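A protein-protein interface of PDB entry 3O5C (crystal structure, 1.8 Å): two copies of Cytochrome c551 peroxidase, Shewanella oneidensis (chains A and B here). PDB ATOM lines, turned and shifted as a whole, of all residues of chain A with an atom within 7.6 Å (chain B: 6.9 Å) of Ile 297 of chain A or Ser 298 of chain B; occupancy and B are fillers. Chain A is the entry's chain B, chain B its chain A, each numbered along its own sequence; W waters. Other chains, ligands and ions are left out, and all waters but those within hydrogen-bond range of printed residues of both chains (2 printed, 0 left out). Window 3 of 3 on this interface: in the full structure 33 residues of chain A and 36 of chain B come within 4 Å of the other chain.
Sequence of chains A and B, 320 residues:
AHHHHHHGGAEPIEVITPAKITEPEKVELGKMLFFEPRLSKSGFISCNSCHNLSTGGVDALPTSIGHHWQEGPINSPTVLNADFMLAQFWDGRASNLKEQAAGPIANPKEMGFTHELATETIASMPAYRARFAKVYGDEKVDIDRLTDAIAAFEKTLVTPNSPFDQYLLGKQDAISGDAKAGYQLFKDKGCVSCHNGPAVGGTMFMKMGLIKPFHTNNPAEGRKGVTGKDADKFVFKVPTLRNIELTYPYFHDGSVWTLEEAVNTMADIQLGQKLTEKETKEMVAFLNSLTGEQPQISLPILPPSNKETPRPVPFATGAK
O of Ile 297 of chain A sits at hydrogen-bond distance from N of Leu 299 of chain B (2.9 Å).
O of Ile 297 of chain B lies within hydrogen-bond range of N of Leu 299 of chain A (3.0 Å).
O of Pro 300 of chain B sits at hydrogen-bond distance from OG of Ser 54 of chain A (2.8 Å).
OG of Ser 298 of chain B is in hydrogen-bond range of NZ of Lys 31 of chain B, 2.5 Å away.
The side-chain amino group (NZ) of Lys 31 of chain A is in hydrogen-bond range of the backbone carbonyl oxygen (O) of Ser 298 of chain A.
Leu 53 of chain A touches Leu 299 of chain B (CB to CD2, 3.5 Å).
CD1 of Ile 301 of chain B touches O of Leu 53 of chain A, at 3.6 Å.
OG of Ser 54 of chain A touches CG of Leu 299 of chain B (3.4 Å).
Ser 54 of chain A touches Ile 301 of chain B (O to C, 3.8 Å).
CB of Gln 294 of chain A touches CD1 of Ile 301 of chain B (3.6 Å).
Ile 301 of chain B touches Pro 295 of chain A.
Ser 298 of chain B touches Gln 296 of chain A (CB to NE2, 3.6 Å).
CA of Ser 298 of chain B touches O of Ile 297 of chain A, at 3.5 Å.
Ser 298 of chain A touches Ile 297 of chain B (CA to O, 3.2 Å).
CD1 of Leu 299 of chain B touches CD1 of Leu 299 of chain A, 3.5 Å away.
Ile 297 of chain A touches just these residues of chain B: Ser 298 (3.5 Å) and Leu 299 (2.9 Å).
Of chain A, only Gln 296 and Ile 297 come within 4 Å of Ser 298 of chain B.
Printed residues of chain A within 4 Å of Ile 297 of chain B: Ser 298 (3.2 Å) and Leu 299 (3.0 Å).
Of the printed residues of chain A, Ile 301 of chain B touches Leu 53 (3.6 Å), Ser 54 (3.8 Å), Gln 294 (3.6 Å) and Pro 295 (3.8 Å).
Thr 156 of chain A touches none of the printed residues of chain B.
The nearest residue of chain B that does not touch Ile 297 of chain A is Ile 297 of chain B (4.1 Å).
The nearest residue of chain A that does not touch Ser 298 of chain B is Ser 298 of chain A (4.3 Å).
The nearest printed residue of chain A that does not touch Ile 297 of chain B is Ile 297 of chain A (4.1 Å).
Hydrophobic or aromatic side chains of chain B within 4 Å of the printed part of chain A: Leu 299, Pro 300 and Ile 301.
Along chain B the printed residues that touch a printed residue of chain A span positions 297 to 301.
Of the 17 printed residues of chain A, 8 touch a printed residue of chain B.
Among the printed residues, no Asp or Glu carboxylate lies within 4 Å of a Lys or Arg side-chain nitrogen of the other chain.
Gln 296 of chain A touches Ser 298 of chain B, but with the chains exchanged Ser 298 of chain A does not touch Gln 296 of chain B (4.2 Å).
Ile 297 of chain A touches Ser 298 of chain B, and with the chains exchanged Ser 298 of chain A touches Ile 297 of chain B.
Ile 297 of chain A touches Leu 299 of chain B, and with the chains exchanged Leu 299 of chain A touches Ile 297 of chain B.
Leu 299 of chain B touches its own counterpart, Leu 299 of chain A.
Positions printed for both chains: 28, 31, 35, 296, 297, 298, 299 and 300.
Of the 13 pairs that touch across the chains among the printed residues, 5 have their exchanged pair printed and touching as well.
Water W2 lies within hydrogen-bond range of the backbone carbonyl oxygen (O) of Leu 299 of chain B (2.6 Å), the backbone carbonyl oxygen (O) of Pro 295 of chain A (2.8 Å) and the backbone NH (N) of Ile 297 of chain A (3.0 Å).
Water W1 lies within hydrogen-bond range of OG of Ser 298 of chain A (2.7 Å), O of Leu 299 of chain A (2.7 Å) and NE2 of Gln 296 of chain B (3.2 Å).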
ATOM      1  N   GLU A  28      15.487  16.048  14.394  1.00  0.00           N
ATOM      2  CA  GLU A  28      15.144  16.952  15.508  1.00  0.00           C
ATOM      3  C   GLU A  28      13.634  17.164  15.618  1.00  0.00           C
ATOM      4  O   GLU A  28      13.083  17.099  16.723  1.00  0.00           O
ATOM      5  CB  GLU A  28      15.840  18.316  15.358  1.00  0.00           C
ATOM      6  CG  GLU A  28      15.560  19.297  16.492  1.00  0.00           C
ATOM      7  CD  GLU A  28      15.948  18.761  17.863  1.00  0.00           C
ATOM      8  OE1 GLU A  28      16.906  17.958  17.940  1.00  0.00           O
ATOM      9  OE2 GLU A  28      15.301  19.163  18.866  1.00  0.00           O
ATOM     10  N   LYS A  31      12.147  14.056  16.896  1.00  0.00           N
ATOM     11  CA  LYS A  31      12.371  13.879  18.324  1.00  0.00           C
ATOM     12  C   LYS A  31      11.364  14.690  19.133  1.00  0.00           C
ATOM     13  O   LYS A  31      10.826  14.195  20.112  1.00  0.00           O
ATOM     14  CB  LYS A  31      13.776  14.267  18.742  1.00  0.00           C
ATOM     15  CG  LYS A  31      13.971  14.181  20.261  1.00  0.00           C
ATOM     16  CD  LYS A  31      15.390  14.451  20.680  1.00  0.00           C
ATOM     17  CE  LYS A  31      15.807  15.894  20.458  1.00  0.00           C
ATOM     18  NZ  LYS A  31      16.951  16.291  21.377  1.00  0.00           N
ATOM     19  N   PHE A  34       7.960  12.908  18.927  1.00  0.00           N
ATOM     20  CA  PHE A  34       7.930  11.677  19.729  1.00  0.00           C
ATOM     21  C   PHE A  34       7.625  11.974  21.216  1.00  0.00           C
ATOM     22  O   PHE A  34       7.040  11.152  21.907  1.00  0.00           O
ATOM     23  CB  PHE A  34       9.274  10.976  19.610  1.00  0.00           C
ATOM     24  CG  PHE A  34       9.311   9.579  20.204  1.00  0.00           C
ATOM     25  CD1 PHE A  34       9.028   8.479  19.422  1.00  0.00           C
ATOM     26  CD2 PHE A  34       9.710   9.378  21.514  1.00  0.00           C
ATOM     27  CE1 PHE A  34       9.109   7.174  19.962  1.00  0.00           C
ATOM     28  CE2 PHE A  34       9.782   8.089  22.065  1.00  0.00           C
ATOM     29  CZ  PHE A  34       9.488   7.006  21.289  1.00  0.00           C
ATOM     30  N   PHE A  35       8.031  13.150  21.681  1.00  0.00           N
ATOM     31  CA  PHE A  35       7.828  13.578  23.076  1.00  0.00           C
ATOM     32  C   PHE A  35       6.670  14.573  23.252  1.00  0.00           C
ATOM     33  O   PHE A  35       6.464  15.119  24.329  1.00  0.00           O
ATOM     34  CB  PHE A  35       9.126  14.215  23.581  1.00  0.00           C
ATOM     35  CG  PHE A  35      10.164  13.217  23.944  1.00  0.00           C
ATOM     36  CD1 PHE A  35      10.340  12.830  25.264  1.00  0.00           C
ATOM     37  CD2 PHE A  35      10.959  12.645  22.972  1.00  0.00           C
ATOM     38  CE1 PHE A  35      11.289  11.896  25.598  1.00  0.00           C
ATOM     39  CE2 PHE A  35      11.906  11.691  23.304  1.00  0.00           C
ATOM     40  CZ  PHE A  35      12.073  11.333  24.630  1.00  0.00           C
ATOM     41  N   LEU A  53      11.918   5.994  26.596  1.00  0.00           N
ATOM     42  CA  LEU A  53      13.317   5.780  26.211  1.00  0.00           C
ATOM     43  C   LEU A  53      14.241   5.690  27.447  1.00  0.00           C
ATOM     44  O   LEU A  53      15.384   5.214  27.352  1.00  0.00           O
ATOM     45  CB  LEU A  53      13.766   6.835  25.205  1.00  0.00           C
ATOM     46  CG  LEU A  53      13.140   6.733  23.802  1.00  0.00           C
ATOM     47  CD1 LEU A  53      13.493   7.947  22.968  1.00  0.00           C
ATOM     48  CD2 LEU A  53      13.590   5.420  23.098  1.00  0.00           C
ATOM     49  N   SER A  54      13.731   6.081  28.617  1.00  0.00           N
ATOM     50  CA  SER A  54      14.464   5.862  29.869  1.00  0.00           C
ATOM     51  C   SER A  54      14.426   4.390  30.322  1.00  0.00           C
ATOM     52  O   SER A  54      15.244   3.985  31.146  1.00  0.00           O
ATOM     53  CB  SER A  54      13.912   6.740  30.982  1.00  0.00           C
ATOM     54  OG  SER A  54      14.003   8.123  30.640  1.00  0.00           O
ATOM     55  N   LEU A  80      13.202   0.468  20.207  1.00  0.00           N
ATOM     56  CA  LEU A  80      14.639   0.263  19.982  1.00  0.00           C
ATOM     57  C   LEU A  80      14.901  -0.821  18.926  1.00  0.00           C
ATOM     58  O   LEU A  80      14.415  -1.962  19.041  1.00  0.00           O
ATOM     59  CB  LEU A  80      15.379  -0.070  21.279  1.00  0.00           C
ATOM     60  CG  LEU A  80      15.314   0.952  22.420  1.00  0.00           C
ATOM     61  CD1 LEU A  80      16.073   0.392  23.620  1.00  0.00           C
ATOM     62  CD2 LEU A  80      15.853   2.350  22.011  1.00  0.00           C
ATOM     63  N   PHE A 153      13.304  10.138  13.212  1.00  0.00           N
ATOM     64  CA  PHE A 153      13.879  10.119  14.564  1.00  0.00           C
ATOM     65  C   PHE A 153      14.066   8.691  15.071  1.00  0.00           C
ATOM     66  O   PHE A 153      15.116   8.352  15.613  1.00  0.00           O
ATOM     67  CB  PHE A 153      13.006  10.914  15.544  1.00  0.00           C
ATOM     68  CG  PHE A 153      13.373  10.701  16.988  1.00  0.00           C
ATOM     69  CD1 PHE A 153      14.581  11.164  17.482  1.00  0.00           C
ATOM     70  CD2 PHE A 153      12.522  10.013  17.845  1.00  0.00           C
ATOM     71  CE1 PHE A 153      14.938  10.953  18.819  1.00  0.00           C
ATOM     72  CE2 PHE A 153      12.877   9.801  19.184  1.00  0.00           C
ATOM     73  CZ  PHE A 153      14.084  10.276  19.664  1.00  0.00           C
ATOM     74  N   THR A 156      17.090   6.583  14.482  1.00  0.00           N
ATOM     75  CA  THR A 156      18.299   6.859  15.259  1.00  0.00           C
ATOM     76  C   THR A 156      18.383   6.010  16.540  1.00  0.00           C
ATOM     77  O   THR A 156      19.455   5.891  17.129  1.00  0.00           O
ATOM     78  CB  THR A 156      18.412   8.357  15.622  1.00  0.00           C
ATOM     79  OG1 THR A 156      17.516   8.668  16.693  1.00  0.00           O
ATOM     80  CG2 THR A 156      18.093   9.235  14.395  1.00  0.00           C
ATOM     81  N   LEU A 157      17.265   5.398  16.939  1.00  0.00           N
ATOM     82  CA  LEU A 157      17.167   4.657  18.198  1.00  0.00           C
ATOM     83  C   LEU A 157      17.660   3.220  18.067  1.00  0.00           C
ATOM     84  O   LEU A 157      16.955   2.285  18.417  1.00  0.00           O
ATOM     85  CB  LEU A 157      15.717   4.661  18.721  1.00  0.00           C
ATOM     86  CG  LEU A 157      15.077   6.043  18.864  1.00  0.00           C
ATOM     87  CD1 LEU A 157      13.620   5.916  19.220  1.00  0.00           C
ATOM     88  CD2 LEU A 157      15.825   6.853  19.915  1.00  0.00           C
ATOM     89  N   GLN A 294      22.017   2.459  25.186  1.00  0.00           N
ATOM     90  CA  GLN A 294      20.697   3.062  25.093  1.00  0.00           C
ATOM     91  C   GLN A 294      20.876   4.457  24.517  1.00  0.00           C
ATOM     92  O   GLN A 294      21.899   5.108  24.768  1.00  0.00           O
ATOM     93  CB  GLN A 294      20.042   3.119  26.479  1.00  0.00           C
ATOM     94  CG  GLN A 294      19.902   1.755  27.165  1.00  0.00           C
ATOM     95  CD  GLN A 294      19.037   0.795  26.376  1.00  0.00           C
ATOM     96  OE1 GLN A 294      17.849   1.049  26.164  1.00  0.00           O
ATOM     97  NE2 GLN A 294      19.622  -0.330  25.944  1.00  0.00           N
ATOM     98  N   PRO A 295      19.915   4.903  23.695  1.00  0.00           N
ATOM     99  CA  PRO A 295      20.004   6.228  23.123  1.00  0.00           C
ATOM    100  C   PRO A 295      20.256   7.331  24.132  1.00  0.00           C
ATOM    101  O   PRO A 295      19.510   7.455  25.116  1.00  0.00           O
ATOM    102  CB  PRO A 295      18.636   6.391  22.470  1.00  0.00           C
ATOM    103  CG  PRO A 295      18.380   5.060  21.924  1.00  0.00           C
ATOM    104  CD  PRO A 295      18.899   4.102  22.989  1.00  0.00           C
ATOM    105  N   GLN A 296      21.300   8.119  23.872  1.00  0.00           N
ATOM    106  CA  GLN A 296      21.607   9.310  24.651  1.00  0.00           C
ATOM    107  C   GLN A 296      21.008  10.499  23.932  1.00  0.00           C
ATOM    108  O   GLN A 296      21.503  10.909  22.888  1.00  0.00           O
ATOM    109  CB  GLN A 296      23.120   9.491  24.808  1.00  0.00           C
ATOM    110  CG  GLN A 296      23.556  10.869  25.349  1.00  0.00           C
ATOM    111  CD  GLN A 296      23.617  10.929  26.856  1.00  0.00           C
ATOM    112  OE1 GLN A 296      24.579  11.445  27.422  1.00  0.00           O
ATOM    113  NE2 GLN A 296      22.601  10.385  27.518  1.00  0.00           N
ATOM    114  N   ILE A 297      19.921  11.021  24.496  1.00  0.00           N
ATOM    115  CA  ILE A 297      19.153  12.081  23.889  1.00  0.00           C
ATOM    116  C   ILE A 297      18.955  13.189  24.908  1.00  0.00           C
ATOM    117  O   ILE A 297      18.729  12.918  26.076  1.00  0.00           O
ATOM    118  CB  ILE A 297      17.794  11.524  23.421  1.00  0.00           C
ATOM    119  CG1 ILE A 297      17.997  10.615  22.201  1.00  0.00           C
ATOM    120  CG2 ILE A 297      16.826  12.612  23.076  1.00  0.00           C
ATOM    121  CD1 ILE A 297      16.753   9.842  21.818  1.00  0.00           C
ATOM    122  N   SER A 298      19.079  14.437  24.470  1.00  0.00           N
ATOM    123  CA  SER A 298      18.687  15.566  25.279  1.00  0.00           C
ATOM    124  C   SER A 298      17.169  15.702  25.175  1.00  0.00           C
ATOM    125  O   SER A 298      16.607  15.575  24.095  1.00  0.00           O
ATOM    126  CB  SER A 298      19.371  16.845  24.801  1.00  0.00           C
ATOM    127  OG  SER A 298      18.848  17.257  23.560  1.00  0.00           O
ATOM    128  N   LEU A 299      16.507  15.956  26.297  1.00  0.00           N
ATOM    129  CA  LEU A 299      15.058  16.159  26.311  1.00  0.00           C
ATOM    130  C   LEU A 299      14.700  17.341  25.420  1.00  0.00           C
ATOM    131  O   LEU A 299      15.289  18.396  25.561  1.00  0.00           O
ATOM    132  CB  LEU A 299      14.572  16.436  27.744  1.00  0.00           C
ATOM    133  CG  LEU A 299      13.097  16.102  27.987  1.00  0.00           C
ATOM    134  CD1 LEU A 299      12.931  14.601  28.099  1.00  0.00           C
ATOM    135  CD2 LEU A 299      12.537  16.809  29.232  1.00  0.00           C
ATOM    136  N   PRO A 300      13.746  17.172  24.490  1.00  0.00           N
ATOM    137  CA  PRO A 300      13.480  18.317  23.627  1.00  0.00           C
ATOM    138  C   PRO A 300      12.658  19.412  24.306  1.00  0.00           C
ATOM    139  O   PRO A 300      11.760  19.119  25.083  1.00  0.00           O
ATOM    140  CB  PRO A 300      12.685  17.703  22.479  1.00  0.00           C
ATOM    141  CG  PRO A 300      12.026  16.525  23.081  1.00  0.00           C
ATOM    142  CD  PRO A 300      12.991  15.981  24.074  1.00  0.00           C
ATOM    143  N   GLU B  28      22.564  13.669  39.262  1.00  0.00           N
ATOM    144  CA  GLU B  28      22.314  12.530  38.374  1.00  0.00           C
ATOM    145  C   GLU B  28      21.271  11.589  38.948  1.00  0.00           C
ATOM    146  O   GLU B  28      20.293  11.223  38.277  1.00  0.00           O
ATOM    147  CB  GLU B  28      23.608  11.745  38.164  1.00  0.00           C
ATOM    148  CG  GLU B  28      24.309  11.973  36.853  1.00  0.00           C
ATOM    149  CD  GLU B  28      24.257  10.733  35.988  1.00  0.00           C
ATOM    150  OE1 GLU B  28      25.196   9.908  36.096  1.00  0.00           O
ATOM    151  OE2 GLU B  28      23.256  10.554  35.251  1.00  0.00           O
ATOM    152  N   LYS B  31      17.911  13.194  38.994  1.00  0.00           N
ATOM    153  CA  LYS B  31      17.296  13.215  37.663  1.00  0.00           C
ATOM    154  C   LYS B  31      16.631  11.891  37.355  1.00  0.00           C
ATOM    155  O   LYS B  31      15.507  11.871  36.905  1.00  0.00           O
ATOM    156  CB  LYS B  31      18.346  13.522  36.598  1.00  0.00           C
ATOM    157  CG  LYS B  31      17.827  13.569  35.192  1.00  0.00           C
ATOM    158  CD  LYS B  31      18.891  14.127  34.252  1.00  0.00           C
ATOM    159  CE  LYS B  31      20.036  13.157  34.009  1.00  0.00           C
ATOM    160  NZ  LYS B  31      20.728  13.553  32.750  1.00  0.00           N
ATOM    161  N   PHE B  35      12.326  11.215  36.828  1.00  0.00           N
ATOM    162  CA  PHE B  35      11.790  10.589  35.611  1.00  0.00           C
ATOM    163  C   PHE B  35      11.416   9.117  35.839  1.00  0.00           C
ATOM    164  O   PHE B  35      11.067   8.424  34.897  1.00  0.00           O
ATOM    165  CB  PHE B  35      12.837  10.656  34.490  1.00  0.00           C
ATOM    166  CG  PHE B  35      12.976  12.024  33.863  1.00  0.00           C
ATOM    167  CD1 PHE B  35      12.216  12.361  32.756  1.00  0.00           C
ATOM    168  CD2 PHE B  35      13.865  12.961  34.377  1.00  0.00           C
ATOM    169  CE1 PHE B  35      12.334  13.605  32.174  1.00  0.00           C
ATOM    170  CE2 PHE B  35      13.987  14.220  33.802  1.00  0.00           C
ATOM    171  CZ  PHE B  35      13.227  14.541  32.695  1.00  0.00           C
ATOM    172  N   GLN B 296      18.780  22.005  29.919  1.00  0.00           N
ATOM    173  CA  GLN B 296      19.373  21.167  28.883  1.00  0.00           C
ATOM    174  C   GLN B 296      19.924  19.909  29.528  1.00  0.00           C
ATOM    175  O   GLN B 296      21.050  19.906  30.038  1.00  0.00           O
ATOM    176  CB  GLN B 296      20.496  21.910  28.142  1.00  0.00           C
ATOM    177  CG  GLN B 296      20.022  22.887  27.069  1.00  0.00           C
ATOM    178  CD  GLN B 296      19.105  22.233  26.037  1.00  0.00           C
ATOM    179  OE1 GLN B 296      18.107  22.823  25.619  1.00  0.00           O
ATOM    180  NE2 GLN B 296      19.433  21.002  25.638  1.00  0.00           N
ATOM    181  N   ILE B 297      19.132  18.844  29.489  1.00  0.00           N
ATOM    182  CA  ILE B 297      19.451  17.620  30.212  1.00  0.00           C
ATOM    183  C   ILE B 297      19.337  16.370  29.360  1.00  0.00           C
ATOM    184  O   ILE B 297      18.595  16.328  28.373  1.00  0.00           O
ATOM    185  CB  ILE B 297      18.531  17.460  31.441  1.00  0.00           C
ATOM    186  CG1 ILE B 297      17.053  17.353  31.038  1.00  0.00           C
ATOM    187  CG2 ILE B 297      18.726  18.633  32.394  1.00  0.00           C
ATOM    188  CD1 ILE B 297      16.317  16.257  31.790  1.00  0.00           C
ATOM    189  N   SER B 298      20.052  15.334  29.775  1.00  0.00           N
ATOM    190  CA  SER B 298      20.042  14.064  29.069  1.00  0.00           C
ATOM    191  C   SER B 298      18.982  13.198  29.715  1.00  0.00           C
ATOM    192  O   SER B 298      18.940  13.062  30.931  1.00  0.00           O
ATOM    193  CB  SER B 298      21.400  13.376  29.152  1.00  0.00           C
ATOM    194  OG  SER B 298      21.745  13.084  30.484  1.00  0.00           O
ATOM    195  N   LEU B 299      18.114  12.641  28.886  1.00  0.00           N
ATOM    196  CA  LEU B 299      17.071  11.754  29.336  1.00  0.00           C
ATOM    197  C   LEU B 299      17.749  10.597  30.061  1.00  0.00           C
ATOM    198  O   LEU B 299      18.588   9.922  29.481  1.00  0.00           O
ATOM    199  CB  LEU B 299      16.273  11.248  28.145  1.00  0.00           C
ATOM    200  CG  LEU B 299      15.036  10.424  28.430  1.00  0.00           C
ATOM    201  CD1 LEU B 299      13.903  11.368  28.864  1.00  0.00           C
ATOM    202  CD2 LEU B 299      14.674   9.607  27.200  1.00  0.00           C
ATOM    203  N   PRO B 300      17.398  10.388  31.340  1.00  0.00           N
ATOM    204  CA  PRO B 300      18.158   9.441  32.153  1.00  0.00           C
ATOM    205  C   PRO B 300      17.838   8.015  31.743  1.00  0.00           C
ATOM    206  O   PRO B 300      16.709   7.726  31.368  1.00  0.00           O
ATOM    207  CB  PRO B 300      17.682   9.745  33.572  1.00  0.00           C
ATOM    208  CG  PRO B 300      16.238  10.239  33.389  1.00  0.00           C
ATOM    209  CD  PRO B 300      16.252  10.969  32.061  1.00  0.00           C
ATOM    210  N   ILE B 301      18.839   7.144  31.785  1.00  0.00           N
ATOM    211  CA  ILE B 301      18.646   5.719  31.530  1.00  0.00           C
ATOM    212  C   ILE B 301      18.510   5.006  32.862  1.00  0.00           C
ATOM    213  O   ILE B 301      19.417   5.038  33.679  1.00  0.00           O
ATOM    214  CB  ILE B 301      19.810   5.122  30.736  1.00  0.00           C
ATOM    215  CG1 ILE B 301      19.969   5.874  29.409  1.00  0.00           C
ATOM    216  CG2 ILE B 301      19.598   3.626  30.493  1.00  0.00           C
ATOM    217  CD1 ILE B 301      18.743   5.845  28.496  1.00  0.00           C
HETATM  218  O   HOH W   1      17.242  19.357  23.927  1.00  0.00           O
HETATM  219  O   HOH W   2      19.046   9.556  26.946  1.00  0.00           O
